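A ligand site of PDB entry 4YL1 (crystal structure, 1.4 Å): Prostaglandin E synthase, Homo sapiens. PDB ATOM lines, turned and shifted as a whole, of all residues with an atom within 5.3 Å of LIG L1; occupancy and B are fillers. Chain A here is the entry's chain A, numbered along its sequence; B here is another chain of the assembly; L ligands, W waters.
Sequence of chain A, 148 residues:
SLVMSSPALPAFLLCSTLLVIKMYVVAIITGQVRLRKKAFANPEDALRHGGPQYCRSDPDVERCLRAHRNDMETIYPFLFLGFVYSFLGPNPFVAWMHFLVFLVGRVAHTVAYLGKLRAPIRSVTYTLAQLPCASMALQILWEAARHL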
ATOM      1  N   ARG A  66      20.277  24.158  19.624  1.00  0.00           N
ATOM      2  CA  ARG A  66      19.573  24.168  18.338  1.00  0.00           C
ATOM      3  C   ARG A  66      20.025  23.019  17.436  1.00  0.00           C
ATOM      4  O   ARG A  66      19.184  22.387  16.789  1.00  0.00           O
ATOM      5  CB  ARG A  66      19.748  25.497  17.600  1.00  0.00           C
ATOM      6  CG  ARG A  66      18.981  26.655  18.223  1.00  0.00           C
ATOM      7  CD  ARG A  66      18.862  27.850  17.292  1.00  0.00           C
ATOM      8  NE  ARG A  66      20.141  28.479  16.955  1.00  0.00           N
ATOM      9  CZ  ARG A  66      20.781  29.349  17.721  1.00  0.00           C
ATOM     10  NH1 ARG A  66      20.273  29.719  18.896  1.00  0.00           N
ATOM     11  NH2 ARG A  66      21.937  29.861  17.310  1.00  0.00           N
ATOM     12  N   ALA A  67      21.333  22.763  17.395  1.00  0.00           N
ATOM     13  CA  ALA A  67      21.854  21.651  16.598  1.00  0.00           C
ATOM     14  C   ALA A  67      21.291  20.329  17.113  1.00  0.00           C
ATOM     15  O   ALA A  67      20.836  19.494  16.330  1.00  0.00           O
ATOM     16  CB  ALA A  67      23.372  21.639  16.606  1.00  0.00           C
ATOM     17  N   ARG A  69      18.545  19.906  18.884  1.00  0.00           N
ATOM     18  CA  ARG A  69      17.123  19.847  18.608  1.00  0.00           C
ATOM     19  C   ARG A  69      16.844  19.497  17.144  1.00  0.00           C
ATOM     20  O   ARG A  69      15.976  18.666  16.852  1.00  0.00           O
ATOM     21  CB  ARG A  69      16.440  21.157  18.985  1.00  0.00           C
ATOM     22  CG  ARG A  69      14.942  21.025  18.965  1.00  0.00           C
ATOM     23  CD  ARG A  69      14.249  22.356  19.171  1.00  0.00           C
ATOM     24  NE  ARG A  69      12.917  22.259  18.582  1.00  0.00           N
ATOM     25  CZ  ARG A  69      11.816  22.740  19.122  1.00  0.00           C
ATOM     26  NH1 ARG A  69      10.676  22.582  18.491  1.00  0.00           N
ATOM     27  NH2 ARG A  69      11.834  23.372  20.292  1.00  0.00           N
ATOM     28  N   ASN A  70      17.581  20.111  16.233  1.00  0.00           N
ATOM     29  CA  ASN A  70      17.402  19.781  14.824  1.00  0.00           C
ATOM     30  C   ASN A  70      17.705  18.300  14.540  1.00  0.00           C
ATOM     31  O   ASN A  70      16.998  17.651  13.780  1.00  0.00           O
ATOM     32  CB  ASN A  70      18.201  20.723  13.923  1.00  0.00           C
ATOM     33  CG  ASN A  70      17.810  20.596  12.470  1.00  0.00           C
ATOM     34  OD1 ASN A  70      18.297  19.722  11.762  1.00  0.00           O
ATOM     35  ND2 ASN A  70      16.910  21.468  12.013  1.00  0.00           N
ATOM     36  N   GLU A  73      14.705  16.383  15.486  1.00  0.00           N
ATOM     37  CA  GLU A  73      13.651  16.597  14.499  1.00  0.00           C
ATOM     38  C   GLU A  73      13.845  15.767  13.215  1.00  0.00           C
ATOM     39  O   GLU A  73      12.890  15.572  12.457  1.00  0.00           O
ATOM     40  CB  GLU A  73      13.549  18.083  14.133  1.00  0.00           C
ATOM     41  CG  GLU A  73      13.072  18.971  15.281  1.00  0.00           C
ATOM     42  CD  GLU A  73      13.201  20.470  15.033  1.00  0.00           C
ATOM     43  OE1 GLU A  73      13.646  20.884  13.942  1.00  0.00           O
ATOM     44  OE2 GLU A  73      12.852  21.254  15.943  1.00  0.00           O
ATOM     45  N   HIS A 109      25.633  18.794   8.386  1.00  0.00           N
ATOM     46  CA  HIS A 109      24.737  19.734   9.064  1.00  0.00           C
ATOM     47  C   HIS A 109      25.311  20.183  10.415  1.00  0.00           C
ATOM     48  O   HIS A 109      25.331  21.376  10.720  1.00  0.00           O
ATOM     49  CB  HIS A 109      23.338  19.123   9.261  1.00  0.00           C
ATOM     50  CG  HIS A 109      22.332  20.082   9.794  1.00  0.00           C
ATOM     51  ND1 HIS A 109      22.152  20.306  11.145  1.00  0.00           N
ATOM     52  CD2 HIS A 109      21.433  20.881   9.165  1.00  0.00           C
ATOM     53  CE1 HIS A 109      21.189  21.192  11.319  1.00  0.00           C
ATOM     54  NE2 HIS A 109      20.735  21.564  10.135  1.00  0.00           N
ATOM     55  N   TYR A 113      26.502  23.843  11.389  1.00  0.00           N
ATOM     56  CA  TYR A 113      25.809  24.535  12.469  1.00  0.00           C
ATOM     57  C   TYR A 113      26.783  24.998  13.551  1.00  0.00           C
ATOM     58  O   TYR A 113      26.862  26.188  13.856  1.00  0.00           O
ATOM     59  CB  TYR A 113      24.730  23.644  13.120  1.00  0.00           C
ATOM     60  CG  TYR A 113      23.476  24.420  13.512  1.00  0.00           C
ATOM     61  CD1 TYR A 113      23.525  25.802  13.704  1.00  0.00           C
ATOM     62  CD2 TYR A 113      22.254  23.774  13.686  1.00  0.00           C
ATOM     63  CE1 TYR A 113      22.391  26.521  14.051  1.00  0.00           C
ATOM     64  CE2 TYR A 113      21.105  24.485  14.027  1.00  0.00           C
ATOM     65  CZ  TYR A 113      21.185  25.859  14.209  1.00  0.00           C
ATOM     66  OH  TYR A 113      20.075  26.597  14.523  1.00  0.00           O
ATOM     67  N   ARG A 122      24.340  25.237   5.817  1.00  0.00           N
ATOM     68  CA  ARG A 122      23.582  24.379   6.745  1.00  0.00           C
ATOM     69  C   ARG A 122      22.230  23.978   6.164  1.00  0.00           C
ATOM     70  O   ARG A 122      21.850  22.802   6.223  1.00  0.00           O
ATOM     71  CB  ARG A 122      23.406  25.074   8.094  1.00  0.00           C
ATOM     72  CG  ARG A 122      22.780  24.176   9.159  1.00  0.00           C
ATOM     73  CD  ARG A 122      22.241  24.995  10.309  1.00  0.00           C
ATOM     74  NE  ARG A 122      21.009  25.706   9.968  1.00  0.00           N
ATOM     75  CZ  ARG A 122      20.905  27.018   9.765  1.00  0.00           C
ATOM     76  NH1 ARG A 122      21.959  27.820   9.872  1.00  0.00           N
ATOM     77  NH2 ARG A 122      19.726  27.528   9.457  1.00  0.00           N
ATOM     78  N   SER A 123      21.505  24.943   5.605  1.00  0.00           N
ATOM     79  CA  SER A 123      20.190  24.673   5.033  1.00  0.00           C
ATOM     80  C   SER A 123      20.236  23.676   3.883  1.00  0.00           C
ATOM     81  O   SER A 123      19.350  22.828   3.755  1.00  0.00           O
ATOM     82  CB  SER A 123      19.535  25.978   4.582  1.00  0.00           C
ATOM     83  OG  SER A 123      19.417  26.882   5.671  1.00  0.00           O
ATOM     84  N   TYR A 126      20.704  20.191   5.367  1.00  0.00           N
ATOM     85  CA  TYR A 126      19.417  19.762   5.911  1.00  0.00           C
ATOM     86  C   TYR A 126      18.510  19.208   4.806  1.00  0.00           C
ATOM     87  O   TYR A 126      17.928  18.128   4.937  1.00  0.00           O
ATOM     88  CB  TYR A 126      18.735  20.924   6.642  1.00  0.00           C
ATOM     89  CG  TYR A 126      17.254  20.731   6.896  1.00  0.00           C
ATOM     90  CD1 TYR A 126      16.796  19.975   7.979  1.00  0.00           C
ATOM     91  CD2 TYR A 126      16.303  21.313   6.055  1.00  0.00           C
ATOM     92  CE1 TYR A 126      15.440  19.811   8.214  1.00  0.00           C
ATOM     93  CE2 TYR A 126      14.937  21.155   6.275  1.00  0.00           C
ATOM     94  CZ  TYR A 126      14.514  20.396   7.358  1.00  0.00           C
ATOM     95  OH  TYR A 126      13.157  20.248   7.576  1.00  0.00           O
ATOM     96  N   ALA B  27       7.855  21.258  10.047  1.00  0.00           N
ATOM     97  CA  ALA B  27       9.183  21.821   9.780  1.00  0.00           C
ATOM     98  C   ALA B  27       9.175  22.768   8.573  1.00  0.00           C
ATOM     99  O   ALA B  27       9.816  23.833   8.621  1.00  0.00           O
ATOM    100  CB  ALA B  27      10.197  20.702   9.568  1.00  0.00           C
ATOM    101  N   THR B  30       7.452  25.986   9.531  1.00  0.00           N
ATOM    102  CA  THR B  30       8.335  26.770  10.399  1.00  0.00           C
ATOM    103  C   THR B  30       9.310  27.609   9.561  1.00  0.00           C
ATOM    104  O   THR B  30       9.469  28.802   9.805  1.00  0.00           O
ATOM    105  CB  THR B  30       9.124  25.863  11.378  1.00  0.00           C
ATOM    106  OG1 THR B  30       8.215  25.065  12.138  1.00  0.00           O
ATOM    107  CG2 THR B  30       9.967  26.708  12.328  1.00  0.00           C
ATOM    108  N   GLY B  31       9.932  26.978   8.570  1.00  0.00           N
ATOM    109  CA  GLY B  31      10.871  27.667   7.681  1.00  0.00           C
ATOM    110  C   GLY B  31      10.201  28.797   6.911  1.00  0.00           C
ATOM    111  O   GLY B  31      10.753  29.896   6.793  1.00  0.00           O
ATOM    112  N   ARG B  34       9.550  31.717   9.270  1.00  0.00           N
ATOM    113  CA  ARG B  34      10.814  32.432   9.522  1.00  0.00           C
ATOM    114  C   ARG B  34      11.124  33.421   8.390  1.00  0.00           C
ATOM    115  O   ARG B  34      11.511  34.551   8.654  1.00  0.00           O
ATOM    116  CB  ARG B  34      11.976  31.457   9.671  1.00  0.00           C
ATOM    117  CG  ARG B  34      11.990  30.678  10.979  1.00  0.00           C
ATOM    118  CD  ARG B  34      13.339  29.990  11.146  1.00  0.00           C
ATOM    119  NE  ARG B  34      13.465  29.233  12.392  1.00  0.00           N
ATOM    120  CZ  ARG B  34      13.728  29.769  13.585  1.00  0.00           C
ATOM    121  NH1 ARG B  34      13.868  31.080  13.720  1.00  0.00           N
ATOM    122  NH2 ARG B  34      13.833  28.984  14.651  1.00  0.00           N
ATOM    123  N   ALA B  41      17.063  32.256  13.603  1.00  0.00           N
ATOM    124  CA  ALA B  41      17.679  31.852  14.860  1.00  0.00           C
ATOM    125  C   ALA B  41      19.181  32.095  14.890  1.00  0.00           C
ATOM    126  O   ALA B  41      19.796  32.081  15.961  1.00  0.00           O
ATOM    127  CB  ALA B  41      17.374  30.388  15.130  1.00  0.00           C
ATOM    128  N   ASN B  42      19.774  32.316  13.715  1.00  0.00           N
ATOM    129  CA  ASN B  42      21.225  32.380  13.583  1.00  0.00           C
ATOM    130  C   ASN B  42      21.668  33.639  12.851  1.00  0.00           C
ATOM    131  O   ASN B  42      21.046  34.007  11.855  1.00  0.00           O
ATOM    132  CB  ASN B  42      21.731  31.165  12.821  1.00  0.00           C
ATOM    133  CG  ASN B  42      21.307  29.866  13.478  1.00  0.00           C
ATOM    134  OD1 ASN B  42      21.721  29.560  14.587  1.00  0.00           O
ATOM    135  ND2 ASN B  42      20.467  29.110  12.789  1.00  0.00           N
ATOM    136  N   LEU B  65       7.547  26.066  16.651  1.00  0.00           N
ATOM    137  CA  LEU B  65       8.496  25.258  17.405  1.00  0.00           C
ATOM    138  C   LEU B  65       7.827  24.489  18.541  1.00  0.00           C
ATOM    139  O   LEU B  65       8.176  23.349  18.821  1.00  0.00           O
ATOM    140  CB  LEU B  65       9.666  26.099  17.918  1.00  0.00           C
ATOM    141  CG  LEU B  65      10.678  26.569  16.872  1.00  0.00           C
ATOM    142  CD1 LEU B  65      11.572  27.640  17.475  1.00  0.00           C
ATOM    143  CD2 LEU B  65      11.512  25.411  16.343  1.00  0.00           C
ATOM    144  N   HIS B  68       5.976  21.543  16.993  1.00  0.00           N
ATOM    145  CA  HIS B  68       6.963  20.529  16.613  1.00  0.00           C
ATOM    146  C   HIS B  68       7.498  19.812  17.851  1.00  0.00           C
ATOM    147  O   HIS B  68       7.645  18.581  17.846  1.00  0.00           O
ATOM    148  CB  HIS B  68       8.101  21.168  15.816  1.00  0.00           C
ATOM    149  CG  HIS B  68       8.821  20.222  14.914  1.00  0.00           C
ATOM    150  ND1 HIS B  68       9.665  20.658  13.913  1.00  0.00           N
ATOM    151  CD2 HIS B  68       8.839  18.867  14.862  1.00  0.00           C
ATOM    152  CE1 HIS B  68      10.166  19.616  13.274  1.00  0.00           C
ATOM    153  NE2 HIS B  68       9.682  18.518  13.828  1.00  0.00           N
HETATM  154  N1  LIG L   1      12.839  23.665  13.655  1.00  0.00           N
HETATM  155  C1  LIG L   1      13.444  24.109  12.364  1.00  0.00           C
HETATM  156  C2  LIG L   1      13.770  25.586  12.391  1.00  0.00           C
HETATM  157  O1  LIG L   1      14.475  26.067  11.478  1.00  0.00           O
HETATM  158  O2  LIG L   1      13.327  26.271  13.338  1.00  0.00           O
HETATM  159  C3  LIG L   1      12.516  23.715  11.215  1.00  0.00           C
HETATM  160  C4  LIG L   1      13.096  23.871   9.806  1.00  0.00           C
HETATM  161  C5  LIG L   1      14.508  23.337   9.691  1.00  0.00           C
HETATM  162  O3  LIG L   1      14.811  22.272  10.184  1.00  0.00           O
HETATM  163  N2  LIG L   1      15.389  24.106   9.036  1.00  0.00           N
HETATM  164  C6  LIG L   1      16.778  23.730   8.854  1.00  0.00           C
HETATM  165  C7  LIG L   1      17.662  24.089  10.019  1.00  0.00           C
HETATM  166  O4  LIG L   1      18.847  23.772   9.996  1.00  0.00           O
HETATM  167  C8  LIG L   1      17.324  24.370   7.580  1.00  0.00           C
HETATM  168  S1  LIG L   1      17.255  26.184   7.612  1.00  0.00           S
HETATM  169  N3  LIG L   1      17.111  24.749  11.037  1.00  0.00           N
HETATM  170  C9  LIG L   1      17.879  25.241  12.171  1.00  0.00           C
HETATM  171  C10 LIG L   1      17.325  24.821  13.513  1.00  0.00           C
HETATM  172  O5  LIG L   1      16.430  23.941  13.563  1.00  0.00           O
HETATM  173  O6  LIG L   1      17.777  25.376  14.534  1.00  0.00           O
HETATM  174  O1  LG2 L   2      15.440  30.033   4.944  1.00  0.00           O
HETATM  175  C1  LG2 L   2      19.406  20.853  -1.956  1.00  0.00           C
HETATM  176  O2  LG2 L   2      19.465  31.033   0.810  1.00  0.00           O
HETATM  177  C2  LG2 L   2      19.343  20.745  -3.362  1.00  0.00           C
HETATM  178  C3  LG2 L   2      18.093  24.621  -0.088  1.00  0.00           C
HETATM  179  N1  LG2 L   2      18.406  28.351   0.451  1.00  0.00           N
HETATM  180  C4  LG2 L   2      19.071  21.937  -4.076  1.00  0.00           C
HETATM  181  C5  LG2 L   2      18.894  23.159  -3.406  1.00  0.00           C
HETATM  182  C6  LG2 L   2      18.965  23.259  -2.008  1.00  0.00           C
HETATM  183  C7  LG2 L   2      18.783  24.547  -1.313  1.00  0.00           C
HETATM  184  O3  LG2 L   2      19.535  31.286  -1.414  1.00  0.00           O
HETATM  185  C8  LG2 L   2      19.288  30.576  -0.459  1.00  0.00           C
HETATM  186  C9  LG2 L   2      19.071  29.145  -0.489  1.00  0.00           C
HETATM  187  C10 LG2 L   2      19.508  28.302  -1.499  1.00  0.00           C
HETATM  188  C11 LG2 L   2      17.637  28.805   1.573  1.00  0.00           C
HETATM  189  C12 LG2 L   2      16.578  29.704   1.407  1.00  0.00           C
HETATM  190  C13 LG2 L   2      15.829  30.129   2.518  1.00  0.00           C
HETATM  191  C14 LG2 L   2      16.122  29.662   3.807  1.00  0.00           C
HETATM  192  C15 LG2 L   2      15.752  29.546   6.263  1.00  0.00           C
HETATM  193  C16 LG2 L   2      16.865  30.385   6.897  1.00  0.00           C
HETATM  194  C17 LG2 L   2      14.474  29.706   7.075  1.00  0.00           C
HETATM  195  C18 LG2 L   2      17.188  28.754   3.965  1.00  0.00           C
HETATM  196  C19 LG2 L   2      17.942  28.327   2.862  1.00  0.00           C
HETATM  197  C20 LG2 L   2      18.434  27.024   0.022  1.00  0.00           C
HETATM  198  C21 LG2 L   2      17.921  25.830   0.587  1.00  0.00           C
HETATM  199  C22 LG2 L   2      19.120  26.982  -1.202  1.00  0.00           C
HETATM  200  C23 LG2 L   2      19.293  25.747  -1.862  1.00  0.00           C
HETATM  201  C24 LG2 L   2      19.232  22.079  -1.299  1.00  0.00           C
HETATM  202  C25 LG2 L   2      19.539  19.385  -4.065  1.00  0.00           C
HETATM  203  C26 LG2 L   2      20.413  19.443  -5.348  1.00  0.00           C
HETATM  204  C27 LG2 L   2      20.230  18.364  -3.137  1.00  0.00           C
HETATM  205  C28 LG2 L   2      18.167  18.814  -4.495  1.00  0.00           C
HETATM  206  O   HOH W   1      13.422  20.066  11.306  1.00  0.00           O
HETATM  207  O   HOH W   2      14.103  26.342   7.283  1.00  0.00           O
HETATM  208  O   HOH W   3      16.370  28.018  13.091  1.00  0.00           O
HETATM  209  O   HOH W   4      10.091  23.415  13.661  1.00  0.00           O
HETATM  210  O   HOH W   5      16.062  27.960  10.238  1.00  0.00           O
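The side-chain carboxylate of Glu 73 lies within salt-bridge range of a nitrogen (N1) of LIG L1 (2.9 Å).
NE of Arg 122 is in hydrogen-bond range of O4 of LIG L1 (2.9 Å).
O2 of LIG L1 is in salt-bridge range of NH2 of Arg 34 of chain B.
ND2 of Asn 70 lies within hydrogen-bond range of O3 of LIG L1 (2.9 Å).
The side-chain hydroxyl of Tyr 113 is in hydrogen-bond range of an oxygen (O6) of LIG L1 (2.6 Å).
NE2 of His 109 is in hydrogen-bond range of O4 of LIG L1 (2.9 Å).
The side-chain hydroxyl (OG) of Ser 123 sits close to a sulfur (S1) of LIG L1, at 3.0 Å.
The guanidinium group (NE) of Arg 66 sits at hydrogen-bond distance from the side-chain hydroxyl (OH) of Tyr 113, at 3.1 Å.
NH1 of Arg 69 sits at hydrogen-bond distance from O of Leu 65 of chain B (2.6 Å).
The side-chain amide oxygen (OD1) of Asn 42 of chain B sits at hydrogen-bond distance from the guanidinium group (NH2) of Arg 66.
NE2 of His 109 sits close to OD1 of Asn 70.
The side-chain hydroxyl (OH) of Tyr 113 lies within hydrogen-bond range of the side-chain amide nitrogen (ND2) of Asn 42 of chain B (3.1 Å).
NH2 of Arg 66 sits at hydrogen-bond distance from O of Ala 41 of chain B, 3.4 Å away.
OE2 of Glu 73 lies within salt-bridge range of NE of Arg 69, at 2.8 Å.
Arg 66 touches LIG L1 (CB to O6, 3.6 Å).
CE1 of Tyr 126 touches O3 of LIG L1, 3.2 Å away.
Ala 27 of chain B touches LIG L1.
Thr 30 of chain B touches LIG L1.
Leu 65 of chain B touches LIG L1.
Hydrophobic or aromatic side chains within 4 Å of LIG L1: His 109, Tyr 113, Tyr 126 and Leu 65 of chain B.
Of the 18 residues printed, 12 come within 4 Å of LIG L1.
The nearest printed residue that does not touch LIG L1 is His 68 of chain B (4.4 Å).
Water W4 lies within hydrogen-bond range of a nitrogen (N1) of LIG L1 (2.8 Å), a ring nitrogen (ND1) of His 68 of chain B (2.8 Å) and the side-chain hydroxyl (OG1) of Thr 30 of chain B (2.9 Å).
Water W1 lies within hydrogen-bond range of the side-chain carboxylate of Glu 73 (2.8 Å) and an oxygen (O3) of LIG L1 (2.8 Å).
Water W3 bridges the guanidinium group (NH2) of Arg 34 of chain B (3.1 Å) and an oxygen (O1) of LIG L1 (3.2 Å).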
